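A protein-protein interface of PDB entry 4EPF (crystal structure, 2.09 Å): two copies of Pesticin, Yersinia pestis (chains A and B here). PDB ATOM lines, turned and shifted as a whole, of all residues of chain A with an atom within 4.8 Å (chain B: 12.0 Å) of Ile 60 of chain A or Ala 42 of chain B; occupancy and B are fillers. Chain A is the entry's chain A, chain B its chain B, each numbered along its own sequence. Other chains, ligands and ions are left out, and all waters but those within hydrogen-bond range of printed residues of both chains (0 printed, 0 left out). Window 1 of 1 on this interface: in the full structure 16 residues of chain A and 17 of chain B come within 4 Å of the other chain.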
ATOM      1  N   LEU A  21       3.124 -12.622  -7.064  1.00  0.00           N
ATOM      2  CA  LEU A  21       4.305 -12.654  -7.947  1.00  0.00           C
ATOM      3  C   LEU A  21       4.778 -11.310  -8.513  1.00  0.00           C
ATOM      4  O   LEU A  21       5.934 -11.186  -8.935  1.00  0.00           O
ATOM      5  CB  LEU A  21       4.060 -13.628  -9.101  1.00  0.00           C
ATOM      6  CG  LEU A  21       5.167 -13.918 -10.112  1.00  0.00           C
ATOM      7  CD1 LEU A  21       6.292 -14.663  -9.476  1.00  0.00           C
ATOM      8  CD2 LEU A  21       4.614 -14.725 -11.272  1.00  0.00           C
ATOM      9  N   PHE A  22       3.893 -10.315  -8.521  1.00  0.00           N
ATOM     10  CA  PHE A  22       4.213  -9.010  -9.087  1.00  0.00           C
ATOM     11  C   PHE A  22       4.125  -7.892  -8.056  1.00  0.00           C
ATOM     12  O   PHE A  22       4.000  -6.722  -8.416  1.00  0.00           O
ATOM     13  CB  PHE A  22       3.270  -8.684 -10.255  1.00  0.00           C
ATOM     14  CG  PHE A  22       3.394  -9.616 -11.425  1.00  0.00           C
ATOM     15  CD1 PHE A  22       4.625  -9.862 -12.013  1.00  0.00           C
ATOM     16  CD2 PHE A  22       2.274 -10.223 -11.954  1.00  0.00           C
ATOM     17  CE1 PHE A  22       4.732 -10.713 -13.094  1.00  0.00           C
ATOM     18  CE2 PHE A  22       2.375 -11.072 -13.039  1.00  0.00           C
ATOM     19  CZ  PHE A  22       3.601 -11.318 -13.607  1.00  0.00           C
ATOM     20  N   ILE A  41       6.032  -3.668 -22.232  1.00  0.00           N
ATOM     21  CA  ILE A  41       6.338  -4.508 -21.070  1.00  0.00           C
ATOM     22  C   ILE A  41       5.308  -5.607 -20.793  1.00  0.00           C
ATOM     23  O   ILE A  41       5.566  -6.516 -19.997  1.00  0.00           O
ATOM     24  CB  ILE A  41       6.541  -3.682 -19.775  1.00  0.00           C
ATOM     25  CG1 ILE A  41       5.213  -3.089 -19.284  1.00  0.00           C
ATOM     26  CG2 ILE A  41       7.620  -2.612 -19.973  1.00  0.00           C
ATOM     27  CD1 ILE A  41       5.085  -3.044 -17.760  1.00  0.00           C
ATOM     28  N   PRO A  44       6.586 -10.736 -22.827  1.00  0.00           N
ATOM     29  CA  PRO A  44       7.832 -11.232 -22.278  1.00  0.00           C
ATOM     30  C   PRO A  44       9.040 -10.717 -23.064  1.00  0.00           C
ATOM     31  O   PRO A  44       9.033 -10.694 -24.294  1.00  0.00           O
ATOM     32  CB  PRO A  44       7.701 -12.750 -22.433  1.00  0.00           C
ATOM     33  CG  PRO A  44       6.250 -12.985 -22.633  1.00  0.00           C
ATOM     34  CD  PRO A  44       5.765 -11.822 -23.382  1.00  0.00           C
ATOM     35  N   MET A  58      13.624 -13.535 -17.843  1.00  0.00           N
ATOM     36  CA  MET A  58      12.411 -13.127 -18.514  1.00  0.00           C
ATOM     37  C   MET A  58      11.793 -11.999 -17.705  1.00  0.00           C
ATOM     38  O   MET A  58      11.555 -12.133 -16.498  1.00  0.00           O
ATOM     39  CB  MET A  58      11.438 -14.303 -18.636  1.00  0.00           C
ATOM     40  CG  MET A  58      10.030 -13.924 -19.126  1.00  0.00           C
ATOM     41  SD  MET A  58       8.793 -15.465 -19.253  1.00  0.00           S
ATOM     42  CE  MET A  58       8.727 -16.030 -17.373  1.00  0.00           C
ATOM     43  N   TYR A  59      11.556 -10.882 -18.382  1.00  0.00           N
ATOM     44  CA  TYR A  59      10.879  -9.734 -17.807  1.00  0.00           C
ATOM     45  C   TYR A  59       9.414  -9.773 -18.220  1.00  0.00           C
ATOM     46  O   TYR A  59       9.083  -9.587 -19.383  1.00  0.00           O
ATOM     47  CB  TYR A  59      11.574  -8.430 -18.232  1.00  0.00           C
ATOM     48  CG  TYR A  59      12.841  -8.152 -17.431  1.00  0.00           C
ATOM     49  CD1 TYR A  59      12.859  -7.179 -16.432  1.00  0.00           C
ATOM     50  CD2 TYR A  59      14.017  -8.889 -17.650  1.00  0.00           C
ATOM     51  CE1 TYR A  59      14.029  -6.936 -15.665  1.00  0.00           C
ATOM     52  CE2 TYR A  59      15.184  -8.663 -16.884  1.00  0.00           C
ATOM     53  CZ  TYR A  59      15.179  -7.683 -15.897  1.00  0.00           C
ATOM     54  OH  TYR A  59      16.322  -7.438 -15.152  1.00  0.00           O
ATOM     55  N   ILE A  60       8.556 -10.099 -17.257  1.00  0.00           N
ATOM     56  CA  ILE A  60       7.106 -10.058 -17.429  1.00  0.00           C
ATOM     57  C   ILE A  60       6.567  -8.906 -16.583  1.00  0.00           C
ATOM     58  O   ILE A  60       6.792  -8.864 -15.368  1.00  0.00           O
ATOM     59  CB  ILE A  60       6.408 -11.355 -16.949  1.00  0.00           C
ATOM     60  CG1 ILE A  60       6.802 -12.562 -17.803  1.00  0.00           C
ATOM     61  CG2 ILE A  60       4.886 -11.170 -16.951  1.00  0.00           C
ATOM     62  CD1 ILE A  60       5.800 -13.743 -17.729  1.00  0.00           C
ATOM     63  N   MET A  61       5.865  -7.977 -17.227  1.00  0.00           N
ATOM     64  CA  MET A  61       5.245  -6.845 -16.540  1.00  0.00           C
ATOM     65  C   MET A  61       6.294  -5.980 -15.856  1.00  0.00           C
ATOM     66  O   MET A  61       6.036  -5.405 -14.801  1.00  0.00           O
ATOM     67  CB  MET A  61       4.209  -7.321 -15.507  1.00  0.00           C
ATOM     68  CG  MET A  61       3.078  -8.199 -16.053  1.00  0.00           C
ATOM     69  SD  MET A  61       1.890  -7.327 -17.348  1.00  0.00           S
ATOM     70  CE  MET A  61       1.587  -5.617 -16.432  1.00  0.00           C
ATOM     71  N   GLY A  62       7.480  -5.904 -16.448  1.00  0.00           N
ATOM     72  CA  GLY A  62       8.561  -5.092 -15.887  1.00  0.00           C
ATOM     73  C   GLY A  62       9.326  -5.731 -14.732  1.00  0.00           C
ATOM     74  O   GLY A  62      10.311  -5.171 -14.259  1.00  0.00           O
ATOM     75  N   PHE A  63       8.884  -6.896 -14.274  1.00  0.00           N
ATOM     76  CA  PHE A  63       9.602  -7.615 -13.223  1.00  0.00           C
ATOM     77  C   PHE A  63      10.456  -8.735 -13.807  1.00  0.00           C
ATOM     78  O   PHE A  63      10.055  -9.358 -14.795  1.00  0.00           O
ATOM     79  CB  PHE A  63       8.627  -8.180 -12.187  1.00  0.00           C
ATOM     80  CG  PHE A  63       7.847  -7.129 -11.457  1.00  0.00           C
ATOM     81  CD1 PHE A  63       8.415  -6.442 -10.390  1.00  0.00           C
ATOM     82  CD2 PHE A  63       6.552  -6.814 -11.844  1.00  0.00           C
ATOM     83  CE1 PHE A  63       7.700  -5.465  -9.709  1.00  0.00           C
ATOM     84  CE2 PHE A  63       5.827  -5.836 -11.174  1.00  0.00           C
ATOM     85  CZ  PHE A  63       6.404  -5.162 -10.102  1.00  0.00           C
ATOM     86  N   ILE A  65      12.050 -12.477 -13.851  1.00  0.00           N
ATOM     87  CA  ILE A  65      11.659 -13.790 -13.398  1.00  0.00           C
ATOM     88  C   ILE A  65      12.701 -14.771 -13.892  1.00  0.00           C
ATOM     89  O   ILE A  65      13.104 -14.758 -15.059  1.00  0.00           O
ATOM     90  CB  ILE A  65      10.238 -14.146 -13.879  1.00  0.00           C
ATOM     91  CG1 ILE A  65       9.207 -13.321 -13.100  1.00  0.00           C
ATOM     92  CG2 ILE A  65       9.952 -15.650 -13.736  1.00  0.00           C
ATOM     93  CD1 ILE A  65       8.012 -12.947 -13.892  1.00  0.00           C
ATOM     94  N   VAL A 111       9.976 -21.499 -10.996  1.00  0.00           N
ATOM     95  CA  VAL A 111       9.658 -20.134 -11.387  1.00  0.00           C
ATOM     96  C   VAL A 111       9.827 -19.265 -10.163  1.00  0.00           C
ATOM     97  O   VAL A 111       9.136 -19.452  -9.155  1.00  0.00           O
ATOM     98  CB  VAL A 111       8.245 -20.030 -11.978  1.00  0.00           C
ATOM     99  CG1 VAL A 111       7.812 -18.588 -12.114  1.00  0.00           C
ATOM    100  CG2 VAL A 111       8.204 -20.723 -13.318  1.00  0.00           C
ATOM    101  N   PRO B  18      -1.688  -2.047 -20.082  1.00  0.00           N
ATOM    102  CA  PRO B  18      -3.079  -2.283 -19.725  1.00  0.00           C
ATOM    103  C   PRO B  18      -3.279  -2.346 -18.221  1.00  0.00           C
ATOM    104  O   PRO B  18      -2.429  -2.881 -17.501  1.00  0.00           O
ATOM    105  CB  PRO B  18      -3.376  -3.649 -20.355  1.00  0.00           C
ATOM    106  CG  PRO B  18      -2.516  -3.691 -21.544  1.00  0.00           C
ATOM    107  CD  PRO B  18      -1.254  -2.928 -21.180  1.00  0.00           C
ATOM    108  N   LEU B  21      -4.734  -6.229 -15.978  1.00  0.00           N
ATOM    109  CA  LEU B  21      -4.661  -7.137 -17.125  1.00  0.00           C
ATOM    110  C   LEU B  21      -4.992  -8.598 -16.798  1.00  0.00           C
ATOM    111  O   LEU B  21      -5.342  -9.377 -17.697  1.00  0.00           O
ATOM    112  CB  LEU B  21      -3.297  -7.017 -17.817  1.00  0.00           C
ATOM    113  CG  LEU B  21      -2.952  -7.895 -19.027  1.00  0.00           C
ATOM    114  CD1 LEU B  21      -3.803  -7.578 -20.237  1.00  0.00           C
ATOM    115  CD2 LEU B  21      -1.485  -7.746 -19.368  1.00  0.00           C
ATOM    116  N   PHE B  22      -4.908  -8.962 -15.521  1.00  0.00           N
ATOM    117  CA  PHE B  22      -5.236 -10.321 -15.097  1.00  0.00           C
ATOM    118  C   PHE B  22      -6.457 -10.403 -14.154  1.00  0.00           C
ATOM    119  O   PHE B  22      -6.716 -11.449 -13.549  1.00  0.00           O
ATOM    120  CB  PHE B  22      -4.001 -10.986 -14.460  1.00  0.00           C
ATOM    121  CG  PHE B  22      -2.758 -10.948 -15.325  1.00  0.00           C
ATOM    122  CD1 PHE B  22      -2.769 -11.455 -16.616  1.00  0.00           C
ATOM    123  CD2 PHE B  22      -1.573 -10.424 -14.830  1.00  0.00           C
ATOM    124  CE1 PHE B  22      -1.624 -11.419 -17.412  1.00  0.00           C
ATOM    125  CE2 PHE B  22      -0.418 -10.394 -15.618  1.00  0.00           C
ATOM    126  CZ  PHE B  22      -0.449 -10.892 -16.910  1.00  0.00           C
ATOM    127  N   ASN B  37       2.913 -29.274 -12.844  1.00  0.00           N
ATOM    128  CA  ASN B  37       1.492 -29.601 -12.735  1.00  0.00           C
ATOM    129  C   ASN B  37       0.603 -28.366 -12.884  1.00  0.00           C
ATOM    130  O   ASN B  37      -0.505 -28.464 -13.427  1.00  0.00           O
ATOM    131  CB  ASN B  37       1.182 -30.326 -11.414  1.00  0.00           C
ATOM    132  CG  ASN B  37       1.899 -31.674 -11.291  1.00  0.00           C
ATOM    133  OD1 ASN B  37       3.123 -31.729 -11.141  1.00  0.00           O
ATOM    134  ND2 ASN B  37       1.129 -32.764 -11.330  1.00  0.00           N
ATOM    135  N   SER B  38       1.081 -27.216 -12.400  1.00  0.00           N
ATOM    136  CA  SER B  38       0.362 -25.933 -12.563  1.00  0.00           C
ATOM    137  C   SER B  38       1.267 -24.691 -12.618  1.00  0.00           C
ATOM    138  O   SER B  38       0.842 -23.640 -13.106  1.00  0.00           O
ATOM    139  CB  SER B  38      -0.713 -25.749 -11.478  1.00  0.00           C
ATOM    140  OG  SER B  38      -1.587 -24.675 -11.806  1.00  0.00           O
ATOM    141  N   ILE B  39       2.499 -24.821 -12.115  1.00  0.00           N
ATOM    142  CA  ILE B  39       3.487 -23.730 -12.098  1.00  0.00           C
ATOM    143  C   ILE B  39       3.752 -23.151 -13.499  1.00  0.00           C
ATOM    144  O   ILE B  39       4.120 -21.984 -13.646  1.00  0.00           O
ATOM    145  CB  ILE B  39       4.817 -24.199 -11.434  1.00  0.00           C
ATOM    146  CG1 ILE B  39       5.646 -23.000 -10.951  1.00  0.00           C
ATOM    147  CG2 ILE B  39       5.610 -25.140 -12.355  1.00  0.00           C
ATOM    148  CD1 ILE B  39       6.958 -23.374 -10.311  1.00  0.00           C
ATOM    149  N   THR B  40       3.524 -23.985 -14.512  1.00  0.00           N
ATOM    150  CA  THR B  40       3.793 -23.680 -15.918  1.00  0.00           C
ATOM    151  C   THR B  40       2.974 -22.533 -16.554  1.00  0.00           C
ATOM    152  O   THR B  40       3.309 -22.081 -17.646  1.00  0.00           O
ATOM    153  CB  THR B  40       3.657 -24.967 -16.787  1.00  0.00           C
ATOM    154  OG1 THR B  40       3.823 -24.644 -18.182  1.00  0.00           O
ATOM    155  CG2 THR B  40       2.285 -25.631 -16.582  1.00  0.00           C
ATOM    156  N   ILE B  41       1.918 -22.062 -15.889  1.00  0.00           N
ATOM    157  CA  ILE B  41       1.102 -20.972 -16.447  1.00  0.00           C
ATOM    158  C   ILE B  41       1.840 -19.632 -16.413  1.00  0.00           C
ATOM    159  O   ILE B  41       1.484 -18.699 -17.135  1.00  0.00           O
ATOM    160  CB  ILE B  41      -0.303 -20.844 -15.780  1.00  0.00           C
ATOM    161  CG1 ILE B  41      -0.201 -20.327 -14.335  1.00  0.00           C
ATOM    162  CG2 ILE B  41      -1.071 -22.174 -15.869  1.00  0.00           C
ATOM    163  CD1 ILE B  41      -1.420 -19.513 -13.865  1.00  0.00           C
ATOM    164  N   ALA B  42       2.867 -19.549 -15.570  1.00  0.00           N
ATOM    165  CA  ALA B  42       3.696 -18.351 -15.461  1.00  0.00           C
ATOM    166  C   ALA B  42       4.650 -18.223 -16.641  1.00  0.00           C
ATOM    167  O   ALA B  42       5.314 -17.199 -16.790  1.00  0.00           O
ATOM    168  CB  ALA B  42       4.458 -18.341 -14.154  1.00  0.00           C
ATOM    169  N   LEU B  43       4.716 -19.266 -17.471  1.00  0.00           N
ATOM    170  CA  LEU B  43       5.466 -19.208 -18.716  1.00  0.00           C
ATOM    171  C   LEU B  43       4.516 -18.897 -19.866  1.00  0.00           C
ATOM    172  O   LEU B  43       3.445 -19.494 -19.963  1.00  0.00           O
ATOM    173  CB  LEU B  43       6.199 -20.524 -18.987  1.00  0.00           C
ATOM    174  CG  LEU B  43       7.478 -20.915 -18.228  1.00  0.00           C
ATOM    175  CD1 LEU B  43       8.450 -19.741 -18.060  1.00  0.00           C
ATOM    176  CD2 LEU B  43       7.176 -21.569 -16.886  1.00  0.00           C
ATOM    177  N   PRO B  44       4.903 -17.957 -20.746  1.00  0.00           N
ATOM    178  CA  PRO B  44       4.058 -17.632 -21.885  1.00  0.00           C
ATOM    179  C   PRO B  44       3.901 -18.819 -22.837  1.00  0.00           C
ATOM    180  O   PRO B  44       4.894 -19.391 -23.288  1.00  0.00           O
ATOM    181  CB  PRO B  44       4.797 -16.472 -22.562  1.00  0.00           C
ATOM    182  CG  PRO B  44       6.208 -16.596 -22.107  1.00  0.00           C
ATOM    183  CD  PRO B  44       6.139 -17.153 -20.725  1.00  0.00           C
ATOM    184  N   HIS B  45       2.650 -19.201 -23.094  1.00  0.00           N
ATOM    185  CA  HIS B  45       2.332 -20.213 -24.092  1.00  0.00           C
ATOM    186  C   HIS B  45       1.648 -19.582 -25.307  1.00  0.00           C
ATOM    187  O   HIS B  45       0.590 -18.970 -25.183  1.00  0.00           O
ATOM    188  CB  HIS B  45       1.475 -21.326 -23.479  1.00  0.00           C
ATOM    189  CG  HIS B  45       2.262 -22.304 -22.663  1.00  0.00           C
ATOM    190  ND1 HIS B  45       2.962 -21.938 -21.532  1.00  0.00           N
ATOM    191  CD2 HIS B  45       2.473 -23.634 -22.821  1.00  0.00           C
ATOM    192  CE1 HIS B  45       3.569 -22.998 -21.029  1.00  0.00           C
ATOM    193  NE2 HIS B  45       3.288 -24.040 -21.792  1.00  0.00           N
ATOM    194  N   TYR B  46       2.288 -19.717 -26.468  1.00  0.00           N
ATOM    195  CA  TYR B  46       1.769 -19.209 -27.730  1.00  0.00           C
ATOM    196  C   TYR B  46       1.088 -20.338 -28.484  1.00  0.00           C
ATOM    197  O   TYR B  46       1.635 -21.435 -28.611  1.00  0.00           O
ATOM    198  CB  TYR B  46       2.897 -18.652 -28.598  1.00  0.00           C
ATOM    199  CG  TYR B  46       3.788 -17.628 -27.926  1.00  0.00           C
ATOM    200  CD1 TYR B  46       3.481 -16.259 -27.977  1.00  0.00           C
ATOM    201  CD2 TYR B  46       4.955 -18.019 -27.263  1.00  0.00           C
ATOM    202  CE1 TYR B  46       4.309 -15.314 -27.371  1.00  0.00           C
ATOM    203  CE2 TYR B  46       5.788 -17.081 -26.653  1.00  0.00           C
ATOM    204  CZ  TYR B  46       5.459 -15.733 -26.711  1.00  0.00           C
ATOM    205  OH  TYR B  46       6.288 -14.810 -26.108  1.00  0.00           O
ATOM    206  N   MET B  58      -1.492 -15.483 -27.137  1.00  0.00           N
ATOM    207  CA  MET B  58      -0.460 -15.722 -26.139  1.00  0.00           C
ATOM    208  C   MET B  58      -1.035 -15.840 -24.730  1.00  0.00           C
ATOM    209  O   MET B  58      -1.613 -14.883 -24.206  1.00  0.00           O
ATOM    210  CB  MET B  58       0.614 -14.642 -26.179  1.00  0.00           C
ATOM    211  CG  MET B  58       1.535 -14.773 -25.014  1.00  0.00           C
ATOM    212  SD  MET B  58       2.705 -13.274 -24.700  1.00  0.00           S
ATOM    213  CE  MET B  58       1.606 -11.764 -25.249  1.00  0.00           C
ATOM    214  N   TYR B  59      -0.868 -17.012 -24.125  1.00  0.00           N
ATOM    215  CA  TYR B  59      -1.339 -17.240 -22.770  1.00  0.00           C
ATOM    216  C   TYR B  59      -0.276 -16.894 -21.723  1.00  0.00           C
ATOM    217  O   TYR B  59       0.732 -17.576 -21.601  1.00  0.00           O
ATOM    218  CB  TYR B  59      -1.835 -18.676 -22.603  1.00  0.00           C
ATOM    219  CG  TYR B  59      -3.151 -18.936 -23.284  1.00  0.00           C
ATOM    220  CD1 TYR B  59      -4.348 -18.927 -22.566  1.00  0.00           C
ATOM    221  CD2 TYR B  59      -3.209 -19.164 -24.656  1.00  0.00           C
ATOM    222  CE1 TYR B  59      -5.578 -19.151 -23.210  1.00  0.00           C
ATOM    223  CE2 TYR B  59      -4.419 -19.395 -25.299  1.00  0.00           C
ATOM    224  CZ  TYR B  59      -5.598 -19.391 -24.576  1.00  0.00           C
ATOM    225  OH  TYR B  59      -6.786 -19.623 -25.240  1.00  0.00           O
ATOM    226  N   ILE B  60      -0.507 -15.805 -20.995  1.00  0.00           N
ATOM    227  CA  ILE B  60       0.327 -15.433 -19.850  1.00  0.00           C
ATOM    228  C   ILE B  60      -0.543 -15.584 -18.609  1.00  0.00           C
ATOM    229  O   ILE B  60      -1.710 -15.178 -18.628  1.00  0.00           O
ATOM    230  CB  ILE B  60       0.784 -13.963 -19.930  1.00  0.00           C
ATOM    231  CG1 ILE B  60       1.365 -13.640 -21.307  1.00  0.00           C
ATOM    232  CG2 ILE B  60       1.807 -13.659 -18.838  1.00  0.00           C
ATOM    233  CD1 ILE B  60       1.467 -12.143 -21.605  1.00  0.00           C
ATOM    234  N   MET B  61       0.008 -16.174 -17.545  1.00  0.00           N
ATOM    235  CA  MET B  61      -0.714 -16.326 -16.271  1.00  0.00           C
ATOM    236  C   MET B  61      -2.056 -17.011 -16.469  1.00  0.00           C
ATOM    237  O   MET B  61      -3.019 -16.747 -15.746  1.00  0.00           O
ATOM    238  CB  MET B  61      -0.918 -14.967 -15.590  1.00  0.00           C
ATOM    239  CG  MET B  61       0.376 -14.270 -15.173  1.00  0.00           C
ATOM    240  SD  MET B  61       1.452 -15.398 -13.987  1.00  0.00           S
ATOM    241  CE  MET B  61       0.208 -15.549 -12.478  1.00  0.00           C
ATOM    242  N   GLY B  62      -2.105 -17.886 -17.468  1.00  0.00           N
ATOM    243  CA  GLY B  62      -3.335 -18.567 -17.851  1.00  0.00           C
ATOM    244  C   GLY B  62      -4.402 -17.703 -18.508  1.00  0.00           C
ATOM    245  O   GLY B  62      -5.556 -18.121 -18.571  1.00  0.00           O
ATOM    246  N   PHE B  63      -4.032 -16.517 -18.997  1.00  0.00           N
ATOM    247  CA  PHE B  63      -4.973 -15.621 -19.697  1.00  0.00           C
ATOM    248  C   PHE B  63      -4.614 -15.412 -21.164  1.00  0.00           C
ATOM    249  O   PHE B  63      -3.442 -15.209 -21.482  1.00  0.00           O
ATOM    250  CB  PHE B  63      -5.072 -14.260 -19.003  1.00  0.00           C
ATOM    251  CG  PHE B  63      -5.759 -14.319 -17.672  1.00  0.00           C
ATOM    252  CD1 PHE B  63      -7.118 -14.593 -17.590  1.00  0.00           C
ATOM    253  CD2 PHE B  63      -5.048 -14.109 -16.498  1.00  0.00           C
ATOM    254  CE1 PHE B  63      -7.759 -14.656 -16.352  1.00  0.00           C
ATOM    255  CE2 PHE B  63      -5.679 -14.170 -15.258  1.00  0.00           C
ATOM    256  CZ  PHE B  63      -7.039 -14.440 -15.189  1.00  0.00           C
ATOM    257  N   PRO B  64      -5.618 -15.488 -22.065  1.00  0.00           N
ATOM    258  CA  PRO B  64      -5.322 -15.234 -23.474  1.00  0.00           C
ATOM    259  C   PRO B  64      -5.056 -13.767 -23.735  1.00  0.00           C
ATOM    260  O   PRO B  64      -5.831 -12.905 -23.318  1.00  0.00           O
ATOM    261  CB  PRO B  64      -6.587 -15.701 -24.218  1.00  0.00           C
ATOM    262  CG  PRO B  64      -7.608 -15.951 -23.199  1.00  0.00           C
ATOM    263  CD  PRO B  64      -7.034 -15.852 -21.837  1.00  0.00           C
ATOM    264  N   ILE B  65      -3.947 -13.493 -24.409  1.00  0.00           N
ATOM    265  CA  ILE B  65      -3.602 -12.133 -24.805  1.00  0.00           C
ATOM    266  C   ILE B  65      -3.470 -12.158 -26.316  1.00  0.00           C
ATOM    267  O   ILE B  65      -2.796 -13.027 -26.885  1.00  0.00           O
ATOM    268  CB  ILE B  65      -2.294 -11.601 -24.116  1.00  0.00           C
ATOM    269  CG1 ILE B  65      -2.538 -11.252 -22.649  1.00  0.00           C
ATOM    270  CG2 ILE B  65      -1.814 -10.322 -24.752  1.00  0.00           C
ATOM    271  CD1 ILE B  65      -2.131 -12.305 -21.696  1.00  0.00           C
ATOM    272  N   THR B  67      -2.155  -9.940 -29.330  1.00  0.00           N
ATOM    273  CA  THR B  67      -1.250  -8.833 -29.628  1.00  0.00           C
ATOM    274  C   THR B  67      -1.065  -8.663 -31.132  1.00  0.00           C
ATOM    275  O   THR B  67      -1.131  -9.635 -31.890  1.00  0.00           O
ATOM    276  CB  THR B  67       0.131  -8.976 -28.920  1.00  0.00           C
ATOM    277  OG1 THR B  67       0.953  -9.935 -29.603  1.00  0.00           O
ATOM    278  CG2 THR B  67      -0.034  -9.377 -27.464  1.00  0.00           C
ATOM    279  N   VAL B 111      -1.897  -4.679 -27.566  1.00  0.00           N
ATOM    280  CA  VAL B 111      -1.939  -5.806 -26.632  1.00  0.00           C
ATOM    281  C   VAL B 111      -3.291  -5.778 -25.920  1.00  0.00           C
ATOM    282  O   VAL B 111      -3.633  -4.799 -25.246  1.00  0.00           O
ATOM    283  CB  VAL B 111      -0.688  -5.848 -25.670  1.00  0.00           C
ATOM    284  CG1 VAL B 111      -0.315  -4.498 -25.213  1.00  0.00           C
ATOM    285  CG2 VAL B 111      -0.924  -6.745 -24.468  1.00  0.00           C
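A ring nitrogen (ND1) of His 45 of chain B lies within hydrogen-bond range of the backbone carbonyl oxygen of Leu 43 of chain B, at 2.9 Å. O of Ile 41 of chain A lies within hydrogen-bond range of N of Met 61 of chain A (3.1 Å). The backbone carbonyl oxygen (O) of Met 58 of chain A lies within hydrogen-bond range of the backbone NH (N) of Ile 65 of chain A. The backbone carbonyl oxygen (O) of Met 58 of chain B is in hydrogen-bond range of the backbone NH (N) of Ile 65 of chain B (2.7 Å).
CG of Pro 44 of chain A touches CG of Pro 44 of chain B, 3.6 Å away. OH of Tyr 46 of chain B touches CG of Pro 44 of chain A (3.9 Å). Pro 44 of chain A touches Met 58 of chain B (CD to SD, 3.6 Å). Ala 42 of chain B touches Met 58 of chain A (O to CE, 3.7 Å). CE of Met 58 of chain A touches CD1 of Leu 43 of chain B, 3.8 Å away. Met 58 of chain A touches Pro 44 of chain B (SD to CD, 3.5 Å). Ile 60 of chain A touches Ala 42 of chain B. Val 111 of chain A touches Ile 39 of chain B (N to CD1, 3.6 Å). Val 111 of chain A touches Ala 42 of chain B (CG1 to CB, 3.9 Å). Val 111 of chain A touches Leu 43 of chain B (CG2 to CD2, 3.8 Å).
Ile 60 of chain A touches just one residue of chain B: Ala 42. Ala 42 of chain B touches just these residues of chain A: Met 58 (3.7 Å), Ile 60 (3.6 Å) and Val 111 (3.9 Å). No residue of chain B comes within 4 Å of Ile 41 of chain A. Met 61 of chain A touches just one residue of chain B: Leu 21. Gly 62 of chain A touches none of the printed residues of chain B. No residue of chain B comes within 4 Å of Phe 63 of chain A. No residue of chain B comes within 4 Å of Ile 65 of chain A. Printed residues of chain A within 4 Å of Tyr 46 of chain B: Pro 44 (3.9 Å). Printed residues of chain A within 4 Å of Leu 43 of chain B: Met 58 (3.8 Å) and Val 111 (3.8 Å). Printed residues of chain A within 4 Å of Ile 39 of chain B: Val 111 (3.6 Å). Printed residues of chain A within 4 Å of Phe 22 of chain B: Phe 22 (3.9 Å). The nearest residue of chain B that does not touch Ile 60 of chain A is Ile 60 of chain B (4.1 Å). The nearest residue of chain A that does not touch Ala 42 of chain B is Leu 21 of chain A (4.6 Å).
Printed residues of chain B that touch a printed residue of chain A: Leu 21, Phe 22, Ile 39, Ala 42, Leu 43, Pro 44, Tyr 46 and Met 58. Hydrophobic or aromatic side chains of chain B within 4 Å of the printed part of chain A: Leu 21, Phe 22, Ile 39, Ala 42, Leu 43, Pro 44, Tyr 46 and Met 58. Of the 12 printed residues of chain A, 6 touch a printed residue of chain B. Printed residues of chain A that touch a printed residue of chain B: Phe 22, Pro 44, Met 58, Ile 60, Met 61 and Val 111. Hydrophobic or aromatic side chains of chain A within 4 Å of the printed part of chain B: Phe 22, Pro 44, Met 58, Ile 60, Met 61 and Val 111. Among the printed residues, 12 pairs touch across the chains. Among the printed residues, no Asp or Glu carboxylate lies within 4 Å of a Lys or Arg side-chain nitrogen of the other chain.
Phe 22 of chain A touches its own counterpart, Phe 22 of chain B. Pro 44 of chain B touches its own counterpart, Pro 44 of chain A. Pro 44 of chain A touches Met 58 of chain B, and with the chains exchanged Met 58 of chain A touches Pro 44 of chain B. Met 61 of chain A touches Leu 21 of chain B, but with the chains exchanged Leu 21 of chain A does not touch Met 61 of chain B (4.2 Å). Of the 12 pairs that touch across the chains among the printed residues, 4 have their exchanged pair printed and touching as well.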
